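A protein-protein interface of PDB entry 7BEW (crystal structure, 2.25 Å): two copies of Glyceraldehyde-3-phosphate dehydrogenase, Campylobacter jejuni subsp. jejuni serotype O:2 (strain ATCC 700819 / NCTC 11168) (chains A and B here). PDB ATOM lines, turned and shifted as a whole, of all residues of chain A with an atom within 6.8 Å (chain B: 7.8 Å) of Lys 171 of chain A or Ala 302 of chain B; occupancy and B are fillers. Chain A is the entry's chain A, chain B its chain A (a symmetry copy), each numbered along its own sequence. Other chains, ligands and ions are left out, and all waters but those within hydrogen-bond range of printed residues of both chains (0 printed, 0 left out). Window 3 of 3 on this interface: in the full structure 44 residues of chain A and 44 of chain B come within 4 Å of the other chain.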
ATOM      1  N   GLY A 168     -17.697  15.811 -23.243  1.00  0.00           N
ATOM      2  CA  GLY A 168     -18.714  14.976 -23.919  1.00  0.00           C
ATOM      3  C   GLY A 168     -18.286  13.518 -23.918  1.00  0.00           C
ATOM      4  O   GLY A 168     -17.149  13.229 -24.416  1.00  0.00           O
ATOM      5  N   ILE A 169     -19.117  12.628 -23.363  1.00  0.00           N
ATOM      6  CA  ILE A 169     -18.846  11.165 -23.382  1.00  0.00           C
ATOM      7  C   ILE A 169     -19.613  10.554 -24.560  1.00  0.00           C
ATOM      8  O   ILE A 169     -20.836  10.716 -24.617  1.00  0.00           O
ATOM      9  CB  ILE A 169     -19.185  10.511 -22.035  1.00  0.00           C
ATOM     10  CG1 ILE A 169     -18.396  11.133 -20.886  1.00  0.00           C
ATOM     11  CG2 ILE A 169     -18.961   9.010 -22.118  1.00  0.00           C
ATOM     12  CD1 ILE A 169     -18.877  10.695 -19.526  1.00  0.00           C
ATOM     13  N   GLU A 170     -18.910   9.926 -25.499  1.00  0.00           N
ATOM     14  CA  GLU A 170     -19.529   9.196 -26.643  1.00  0.00           C
ATOM     15  C   GLU A 170     -19.876   7.780 -26.175  1.00  0.00           C
ATOM     16  O   GLU A 170     -20.978   7.322 -26.458  1.00  0.00           O
ATOM     17  CB  GLU A 170     -18.602   9.186 -27.862  1.00  0.00           C
ATOM     18  CG  GLU A 170     -18.403  10.577 -28.474  1.00  0.00           C
ATOM     19  CD  GLU A 170     -19.650  11.209 -29.100  1.00  0.00           C
ATOM     20  OE1 GLU A 170     -20.449  10.475 -29.689  1.00  0.00           O
ATOM     21  OE2 GLU A 170     -19.831  12.430 -28.993  1.00  0.00           O
ATOM     22  N   LYS A 171     -18.958   7.099 -25.500  1.00  0.00           N
ATOM     23  CA  LYS A 171     -19.213   5.731 -24.999  1.00  0.00           C
ATOM     24  C   LYS A 171     -18.102   5.373 -24.019  1.00  0.00           C
ATOM     25  O   LYS A 171     -17.125   6.095 -23.986  1.00  0.00           O
ATOM     26  CB  LYS A 171     -19.277   4.742 -26.161  1.00  0.00           C
ATOM     27  CG  LYS A 171     -18.069   4.787 -27.083  1.00  0.00           C
ATOM     28  CD  LYS A 171     -18.239   4.033 -28.378  1.00  0.00           C
ATOM     29  CE  LYS A 171     -18.867   4.864 -29.472  1.00  0.00           C
ATOM     30  NZ  LYS A 171     -18.508   4.375 -30.825  1.00  0.00           N
ATOM     31  N   GLY A 172     -18.293   4.332 -23.222  1.00  0.00           N
ATOM     32  CA  GLY A 172     -17.361   3.988 -22.137  1.00  0.00           C
ATOM     33  C   GLY A 172     -17.680   2.659 -21.489  1.00  0.00           C
ATOM     34  O   GLY A 172     -18.856   2.271 -21.458  1.00  0.00           O
ATOM     35  N   LEU A 173     -16.645   1.974 -21.016  1.00  0.00           N
ATOM     36  CA  LEU A 173     -16.790   0.749 -20.217  1.00  0.00           C
ATOM     37  C   LEU A 173     -15.937   0.915 -18.968  1.00  0.00           C
ATOM     38  O   LEU A 173     -14.929   1.614 -18.977  1.00  0.00           O
ATOM     39  CB  LEU A 173     -16.389  -0.483 -21.034  1.00  0.00           C
ATOM     40  CG  LEU A 173     -17.292  -0.823 -22.220  1.00  0.00           C
ATOM     41  CD1 LEU A 173     -16.628  -1.807 -23.191  1.00  0.00           C
ATOM     42  CD2 LEU A 173     -18.630  -1.348 -21.729  1.00  0.00           C
ATOM     43  N   GLY A 224     -27.517   4.230 -22.595  1.00  0.00           N
ATOM     44  CA  GLY A 224     -26.989   3.330 -23.649  1.00  0.00           C
ATOM     45  C   GLY A 224     -25.523   3.557 -23.989  1.00  0.00           C
ATOM     46  O   GLY A 224     -25.014   2.897 -24.915  1.00  0.00           O
ATOM     47  N   LYS A 225     -24.836   4.428 -23.254  1.00  0.00           N
ATOM     48  CA  LYS A 225     -23.458   4.834 -23.604  1.00  0.00           C
ATOM     49  C   LYS A 225     -22.417   4.179 -22.685  1.00  0.00           C
ATOM     50  O   LYS A 225     -21.273   4.163 -23.108  1.00  0.00           O
ATOM     51  CB  LYS A 225     -23.363   6.354 -23.587  1.00  0.00           C
ATOM     52  CG  LYS A 225     -23.911   7.087 -24.818  1.00  0.00           C
ATOM     53  CD  LYS A 225     -23.611   8.586 -24.662  1.00  0.00           C
ATOM     54  CE  LYS A 225     -24.510   9.544 -25.419  1.00  0.00           C
ATOM     55  NZ  LYS A 225     -24.484   9.259 -26.858  1.00  0.00           N
ATOM     56  N   LEU A 226     -22.782   3.687 -21.500  1.00  0.00           N
ATOM     57  CA  LEU A 226     -21.851   3.085 -20.503  1.00  0.00           C
ATOM     58  C   LEU A 226     -22.348   1.706 -20.093  1.00  0.00           C
ATOM     59  O   LEU A 226     -23.559   1.505 -19.945  1.00  0.00           O
ATOM     60  CB  LEU A 226     -21.732   3.938 -19.242  1.00  0.00           C
ATOM     61  CG  LEU A 226     -21.285   5.384 -19.431  1.00  0.00           C
ATOM     62  CD1 LEU A 226     -21.086   6.044 -18.074  1.00  0.00           C
ATOM     63  CD2 LEU A 226     -20.010   5.522 -20.262  1.00  0.00           C
ATOM     64  N   LEU A 243     -12.425   3.787 -15.491  1.00  0.00           N
ATOM     65  CA  LEU A 243     -13.325   4.175 -16.594  1.00  0.00           C
ATOM     66  C   LEU A 243     -12.516   4.339 -17.868  1.00  0.00           C
ATOM     67  O   LEU A 243     -11.668   5.214 -17.902  1.00  0.00           O
ATOM     68  CB  LEU A 243     -13.995   5.505 -16.255  1.00  0.00           C
ATOM     69  CG  LEU A 243     -14.931   5.990 -17.349  1.00  0.00           C
ATOM     70  CD1 LEU A 243     -16.042   4.960 -17.592  1.00  0.00           C
ATOM     71  CD2 LEU A 243     -15.500   7.362 -17.011  1.00  0.00           C
ATOM     72  N   THR A 244     -12.885   3.610 -18.907  1.00  0.00           N
ATOM     73  CA  THR A 244     -12.320   3.783 -20.250  1.00  0.00           C
ATOM     74  C   THR A 244     -13.408   4.351 -21.156  1.00  0.00           C
ATOM     75  O   THR A 244     -14.445   3.775 -21.257  1.00  0.00           O
ATOM     76  CB  THR A 244     -11.701   2.476 -20.735  1.00  0.00           C
ATOM     77  OG1 THR A 244     -10.822   1.944 -19.741  1.00  0.00           O
ATOM     78  CG2 THR A 244     -10.922   2.690 -22.013  1.00  0.00           C
ATOM     79  N   ALA A 245     -13.176   5.473 -21.811  1.00  0.00           N
ATOM     80  CA  ALA A 245     -14.232   6.127 -22.598  1.00  0.00           C
ATOM     81  C   ALA A 245     -13.660   6.784 -23.842  1.00  0.00           C
ATOM     82  O   ALA A 245     -12.470   7.080 -23.877  1.00  0.00           O
ATOM     83  CB  ALA A 245     -14.938   7.137 -21.741  1.00  0.00           C
ATOM     84  N   GLN A 246     -14.531   6.987 -24.823  1.00  0.00           N
ATOM     85  CA  GLN A 246     -14.272   7.810 -26.024  1.00  0.00           C
ATOM     86  C   GLN A 246     -15.014   9.123 -25.777  1.00  0.00           C
ATOM     87  O   GLN A 246     -16.213   9.068 -25.521  1.00  0.00           O
ATOM     88  CB  GLN A 246     -14.692   7.052 -27.284  1.00  0.00           C
ATOM     89  CG  GLN A 246     -14.541   7.866 -28.568  1.00  0.00           C
ATOM     90  CD  GLN A 246     -15.373   7.378 -29.741  1.00  0.00           C
ATOM     91  OE1 GLN A 246     -15.975   6.301 -29.726  1.00  0.00           O
ATOM     92  NE2 GLN A 246     -15.407   8.183 -30.796  1.00  0.00           N
ATOM     93  N   LEU A 247     -14.289  10.241 -25.732  1.00  0.00           N
ATOM     94  CA  LEU A 247     -14.851  11.609 -25.594  1.00  0.00           C
ATOM     95  C   LEU A 247     -15.195  12.197 -26.974  1.00  0.00           C
ATOM     96  O   LEU A 247     -14.635  11.743 -27.961  1.00  0.00           O
ATOM     97  CB  LEU A 247     -13.852  12.487 -24.841  1.00  0.00           C
ATOM     98  CG  LEU A 247     -13.424  11.934 -23.487  1.00  0.00           C
ATOM     99  CD1 LEU A 247     -12.715  12.989 -22.656  1.00  0.00           C
ATOM    100  CD2 LEU A 247     -14.605  11.393 -22.723  1.00  0.00           C
ATOM    101  N   ALA B 245     -10.992  -1.584 -26.031  1.00  0.00           N
ATOM    102  CA  ALA B 245     -10.527  -1.157 -27.360  1.00  0.00           C
ATOM    103  C   ALA B 245     -11.693  -0.731 -28.236  1.00  0.00           C
ATOM    104  O   ALA B 245     -12.821  -1.139 -27.981  1.00  0.00           O
ATOM    105  CB  ALA B 245      -9.762  -2.276 -28.004  1.00  0.00           C
ATOM    106  N   GLN B 246     -11.378   0.081 -29.238  1.00  0.00           N
ATOM    107  CA  GLN B 246     -12.284   0.440 -30.349  1.00  0.00           C
ATOM    108  C   GLN B 246     -11.806  -0.390 -31.540  1.00  0.00           C
ATOM    109  O   GLN B 246     -10.629  -0.295 -31.873  1.00  0.00           O
ATOM    110  CB  GLN B 246     -12.277   1.954 -30.566  1.00  0.00           C
ATOM    111  CG  GLN B 246     -13.121   2.406 -31.758  1.00  0.00           C
ATOM    112  CD  GLN B 246     -12.773   3.776 -32.311  1.00  0.00           C
ATOM    113  OE1 GLN B 246     -12.005   4.551 -31.733  1.00  0.00           O
ATOM    114  NE2 GLN B 246     -13.356   4.098 -33.459  1.00  0.00           N
ATOM    115  N   LEU B 247     -12.666  -1.261 -32.068  1.00  0.00           N
ATOM    116  CA  LEU B 247     -12.404  -2.080 -33.279  1.00  0.00           C
ATOM    117  C   LEU B 247     -12.803  -1.312 -34.551  1.00  0.00           C
ATOM    118  O   LEU B 247     -13.614  -0.401 -34.457  1.00  0.00           O
ATOM    119  CB  LEU B 247     -13.160  -3.403 -33.161  1.00  0.00           C
ATOM    120  CG  LEU B 247     -12.854  -4.191 -31.893  1.00  0.00           C
ATOM    121  CD1 LEU B 247     -13.358  -5.620 -31.992  1.00  0.00           C
ATOM    122  CD2 LEU B 247     -11.376  -4.192 -31.597  1.00  0.00           C
ATOM    123  N   ARG B 249     -14.599  -2.192 -36.976  1.00  0.00           N
ATOM    124  CA  ARG B 249     -15.994  -2.424 -37.431  1.00  0.00           C
ATOM    125  C   ARG B 249     -16.896  -2.849 -36.276  1.00  0.00           C
ATOM    126  O   ARG B 249     -16.400  -3.124 -35.167  1.00  0.00           O
ATOM    127  CB  ARG B 249     -16.033  -3.499 -38.515  1.00  0.00           C
ATOM    128  CG  ARG B 249     -15.755  -4.905 -38.007  1.00  0.00           C
ATOM    129  CD  ARG B 249     -16.250  -5.862 -39.062  1.00  0.00           C
ATOM    130  NE  ARG B 249     -15.867  -7.254 -38.944  1.00  0.00           N
ATOM    131  CZ  ARG B 249     -16.578  -8.193 -38.325  1.00  0.00           C
ATOM    132  NH1 ARG B 249     -17.678  -7.892 -37.651  1.00  0.00           N
ATOM    133  NH2 ARG B 249     -16.146  -9.441 -38.362  1.00  0.00           N
ATOM    134  N   LYS B 250     -18.190  -2.886 -36.554  1.00  0.00           N
ATOM    135  CA  LYS B 250     -19.225  -3.331 -35.595  1.00  0.00           C
ATOM    136  C   LYS B 250     -19.047  -4.831 -35.354  1.00  0.00           C
ATOM    137  O   LYS B 250     -18.822  -5.550 -36.329  1.00  0.00           O
ATOM    138  CB  LYS B 250     -20.633  -3.008 -36.112  1.00  0.00           C
ATOM    139  CG  LYS B 250     -21.763  -3.637 -35.316  1.00  0.00           C
ATOM    140  CD  LYS B 250     -23.060  -2.839 -35.392  1.00  0.00           C
ATOM    141  CE  LYS B 250     -24.161  -3.348 -34.468  1.00  0.00           C
ATOM    142  NZ  LYS B 250     -25.487  -2.845 -34.903  1.00  0.00           N
ATOM    143  N   VAL B 251     -19.127  -5.263 -34.092  1.00  0.00           N
ATOM    144  CA  VAL B 251     -19.018  -6.691 -33.700  1.00  0.00           C
ATOM    145  C   VAL B 251     -20.077  -6.932 -32.643  1.00  0.00           C
ATOM    146  O   VAL B 251     -20.524  -5.948 -32.044  1.00  0.00           O
ATOM    147  CB  VAL B 251     -17.611  -7.042 -33.172  1.00  0.00           C
ATOM    148  CG1 VAL B 251     -16.519  -6.771 -34.196  1.00  0.00           C
ATOM    149  CG2 VAL B 251     -17.322  -6.302 -31.890  1.00  0.00           C
ATOM    150  N   VAL B 300     -19.593  -5.398 -25.192  1.00  0.00           N
ATOM    151  CA  VAL B 300     -19.571  -4.500 -26.379  1.00  0.00           C
ATOM    152  C   VAL B 300     -20.604  -3.445 -26.087  1.00  0.00           C
ATOM    153  O   VAL B 300     -21.705  -3.815 -25.650  1.00  0.00           O
ATOM    154  CB  VAL B 300     -19.939  -5.189 -27.702  1.00  0.00           C
ATOM    155  CG1 VAL B 300     -19.846  -4.227 -28.884  1.00  0.00           C
ATOM    156  CG2 VAL B 300     -19.090  -6.417 -27.940  1.00  0.00           C
ATOM    157  N   ILE B 301     -20.242  -2.196 -26.324  1.00  0.00           N
ATOM    158  CA  ILE B 301     -21.222  -1.097 -26.294  1.00  0.00           C
ATOM    159  C   ILE B 301     -21.014  -0.248 -27.544  1.00  0.00           C
ATOM    160  O   ILE B 301     -19.864  -0.167 -28.036  1.00  0.00           O
ATOM    161  CB  ILE B 301     -21.115  -0.323 -24.969  1.00  0.00           C
ATOM    162  CG1 ILE B 301     -22.338   0.568 -24.753  1.00  0.00           C
ATOM    163  CG2 ILE B 301     -19.825   0.466 -24.867  1.00  0.00           C
ATOM    164  CD1 ILE B 301     -23.026   0.325 -23.461  1.00  0.00           C
ATOM    165  N   ALA B 302     -22.125   0.279 -28.056  1.00  0.00           N
ATOM    166  CA  ALA B 302     -22.196   1.261 -29.155  1.00  0.00           C
ATOM    167  C   ALA B 302     -21.375   0.755 -30.346  1.00  0.00           C
ATOM    168  O   ALA B 302     -20.548   1.534 -30.854  1.00  0.00           O
ATOM    169  CB  ALA B 302     -21.707   2.580 -28.630  1.00  0.00           C
ATOM    170  N   ASP B 303     -21.547  -0.522 -30.681  1.00  0.00           N
ATOM    171  CA  ASP B 303     -21.157  -1.187 -31.957  1.00  0.00           C
ATOM    172  C   ASP B 303     -19.722  -1.736 -31.876  1.00  0.00           C
ATOM    173  O   ASP B 303     -19.508  -2.917 -32.232  1.00  0.00           O
ATOM    174  CB  ASP B 303     -21.308  -0.244 -33.161  1.00  0.00           C
ATOM    175  CG  ASP B 303     -22.733   0.197 -33.501  1.00  0.00           C
ATOM    176  OD1 ASP B 303     -23.693  -0.437 -32.989  1.00  0.00           O
ATOM    177  OD2 ASP B 303     -22.880   1.158 -34.323  1.00  0.00           O
ATOM    178  N   ASP B 304     -18.758  -0.884 -31.519  1.00  0.00           N
ATOM    179  CA  ASP B 304     -17.324  -1.123 -31.790  1.00  0.00           C
ATOM    180  C   ASP B 304     -16.455  -0.933 -30.534  1.00  0.00           C
ATOM    181  O   ASP B 304     -15.246  -0.984 -30.646  1.00  0.00           O
ATOM    182  CB  ASP B 304     -16.918  -0.215 -32.947  1.00  0.00           C
ATOM    183  CG  ASP B 304     -16.836   1.276 -32.627  1.00  0.00           C
ATOM    184  OD1 ASP B 304     -17.220   1.698 -31.498  1.00  0.00           O
ATOM    185  OD2 ASP B 304     -16.352   2.008 -33.512  1.00  0.00           O
ATOM    186  N   PHE B 305     -17.032  -0.683 -29.373  1.00  0.00           N
ATOM    187  CA  PHE B 305     -16.266  -0.378 -28.150  1.00  0.00           C
ATOM    188  C   PHE B 305     -16.333  -1.618 -27.257  1.00  0.00           C
ATOM    189  O   PHE B 305     -17.448  -1.956 -26.840  1.00  0.00           O
ATOM    190  CB  PHE B 305     -16.853   0.874 -27.513  1.00  0.00           C
ATOM    191  CG  PHE B 305     -15.956   1.535 -26.504  1.00  0.00           C
ATOM    192  CD1 PHE B 305     -15.937   1.099 -25.196  1.00  0.00           C
ATOM    193  CD2 PHE B 305     -15.144   2.596 -26.862  1.00  0.00           C
ATOM    194  CE1 PHE B 305     -15.099   1.689 -24.266  1.00  0.00           C
ATOM    195  CE2 PHE B 305     -14.325   3.201 -25.923  1.00  0.00           C
ATOM    196  CZ  PHE B 305     -14.323   2.763 -24.622  1.00  0.00           C
ATOM    197  N   ILE B 306     -15.218  -2.308 -27.041  1.00  0.00           N
ATOM    198  CA  ILE B 306     -15.253  -3.667 -26.428  1.00  0.00           C
ATOM    199  C   ILE B 306     -14.387  -3.699 -25.179  1.00  0.00           C
ATOM    200  O   ILE B 306     -13.441  -2.899 -25.096  1.00  0.00           O
ATOM    201  CB  ILE B 306     -14.794  -4.737 -27.429  1.00  0.00           C
ATOM    202  CG1 ILE B 306     -13.280  -4.678 -27.645  1.00  0.00           C
ATOM    203  CG2 ILE B 306     -15.574  -4.593 -28.728  1.00  0.00           C
ATOM    204  CD1 ILE B 306     -12.676  -5.950 -28.131  1.00  0.00           C
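Positions printed for both chains: 245, 246 and 247.
The side-chain amino group (NZ) of Lys 171 of chain A sits at hydrogen-bond distance from the backbone carbonyl oxygen (O) of Ala 302 of chain B.
The side-chain amino group (NZ) of Lys 171 of chain A lies within salt-bridge range of the side-chain carboxylate (OD1) of Asp 304 of chain B (3.0 Å).
Printed residues of chain A that touch a printed residue of chain B: Lys 171, Gly 172, Leu 173, Gly 224, Lys 225, Leu 226, Thr 244, Ala 245 and Gln 246.
Hydrophobic or aromatic side chains of chain A that line the printed part of chain B: Leu 173.
Of the 13 printed residues of chain B, 5 touch a printed residue of chain A.
Hydrophobic or aromatic side chains of chain B that line the printed part of chain A: Ile 301, Ala 302 and Phe 305.
Along chain B the printed residues that touch a printed residue of chain A span positions 301 to 306.
Among the printed residues, 14 pairs touch across the chains.
Among the printed residues, Asp or Glu carboxylates within 4 Å of a Lys or Arg side-chain nitrogen of the other chain: Lys 171 of chain A with Asp 304 of chain B.
Among the printed residues, pairs that only touch across the chains: Lys 171 of chain A with Phe 305 of chain B, Gly 172 of chain A with Ile 301 of chain B, Gly 172 of chain A with Phe 305 of chain B, Leu 173 of chain A with Ile 301 of chain B, Leu 173 of chain A with Phe 305 of chain B, Leu 173 of chain A with Ile 306 of chain B, Gly 224 of chain A with Ile 301 of chain B, Lys 225 of chain A with Ile 301 of chain B, Leu 226 of chain A with Ile 301 of chain B, Thr 244 of chain A with Phe 305 of chain B, Ala 245 of chain A with Phe 305 of chain B and Gln 246 of chain A with Phe 305 of chain B.
The backbone NH of Glu 170 of chain A sits at hydrogen-bond distance from the backbone carbonyl oxygen of Gln 246 of chain A (2.8 Å).
O of Lys 171 of chain A lies within hydrogen-bond range of N of Gln 246 of chain A, at 2.9 Å.
The backbone carbonyl oxygen (O) of Lys 225 of chain A is in hydrogen-bond range of the backbone NH (N) of Gly 172 of chain A, 3.0 Å away.
The backbone NH of Leu 173 of chain A is in hydrogen-bond range of the backbone carbonyl oxygen of Thr 244 of chain A (2.9 Å).
The backbone carbonyl oxygen (O) of Ala 245 of chain B is in hydrogen-bond range of the backbone NH (N) of Ile 306 of chain B (2.8 Å).
N of Leu 247 of chain B sits at hydrogen-bond distance from O of Asp 304 of chain B (3.0 Å).
Printed residues of chain B within 4 Å of Gly 172 of chain A: Ile 301 and Phe 305.
Printed residues of chain B within 4 Å of Thr 244 of chain A: Phe 305 (3.5 Å).
Arg 249 of chain B touches none of the printed residues of chain A.
Of chain A, only Lys 171 comes within 4 Å of Ala 302 of chain B.
The nearest printed residue of chain B that does not touch Gly 172 of chain A is Ala 302 of chain B (6.6 Å).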
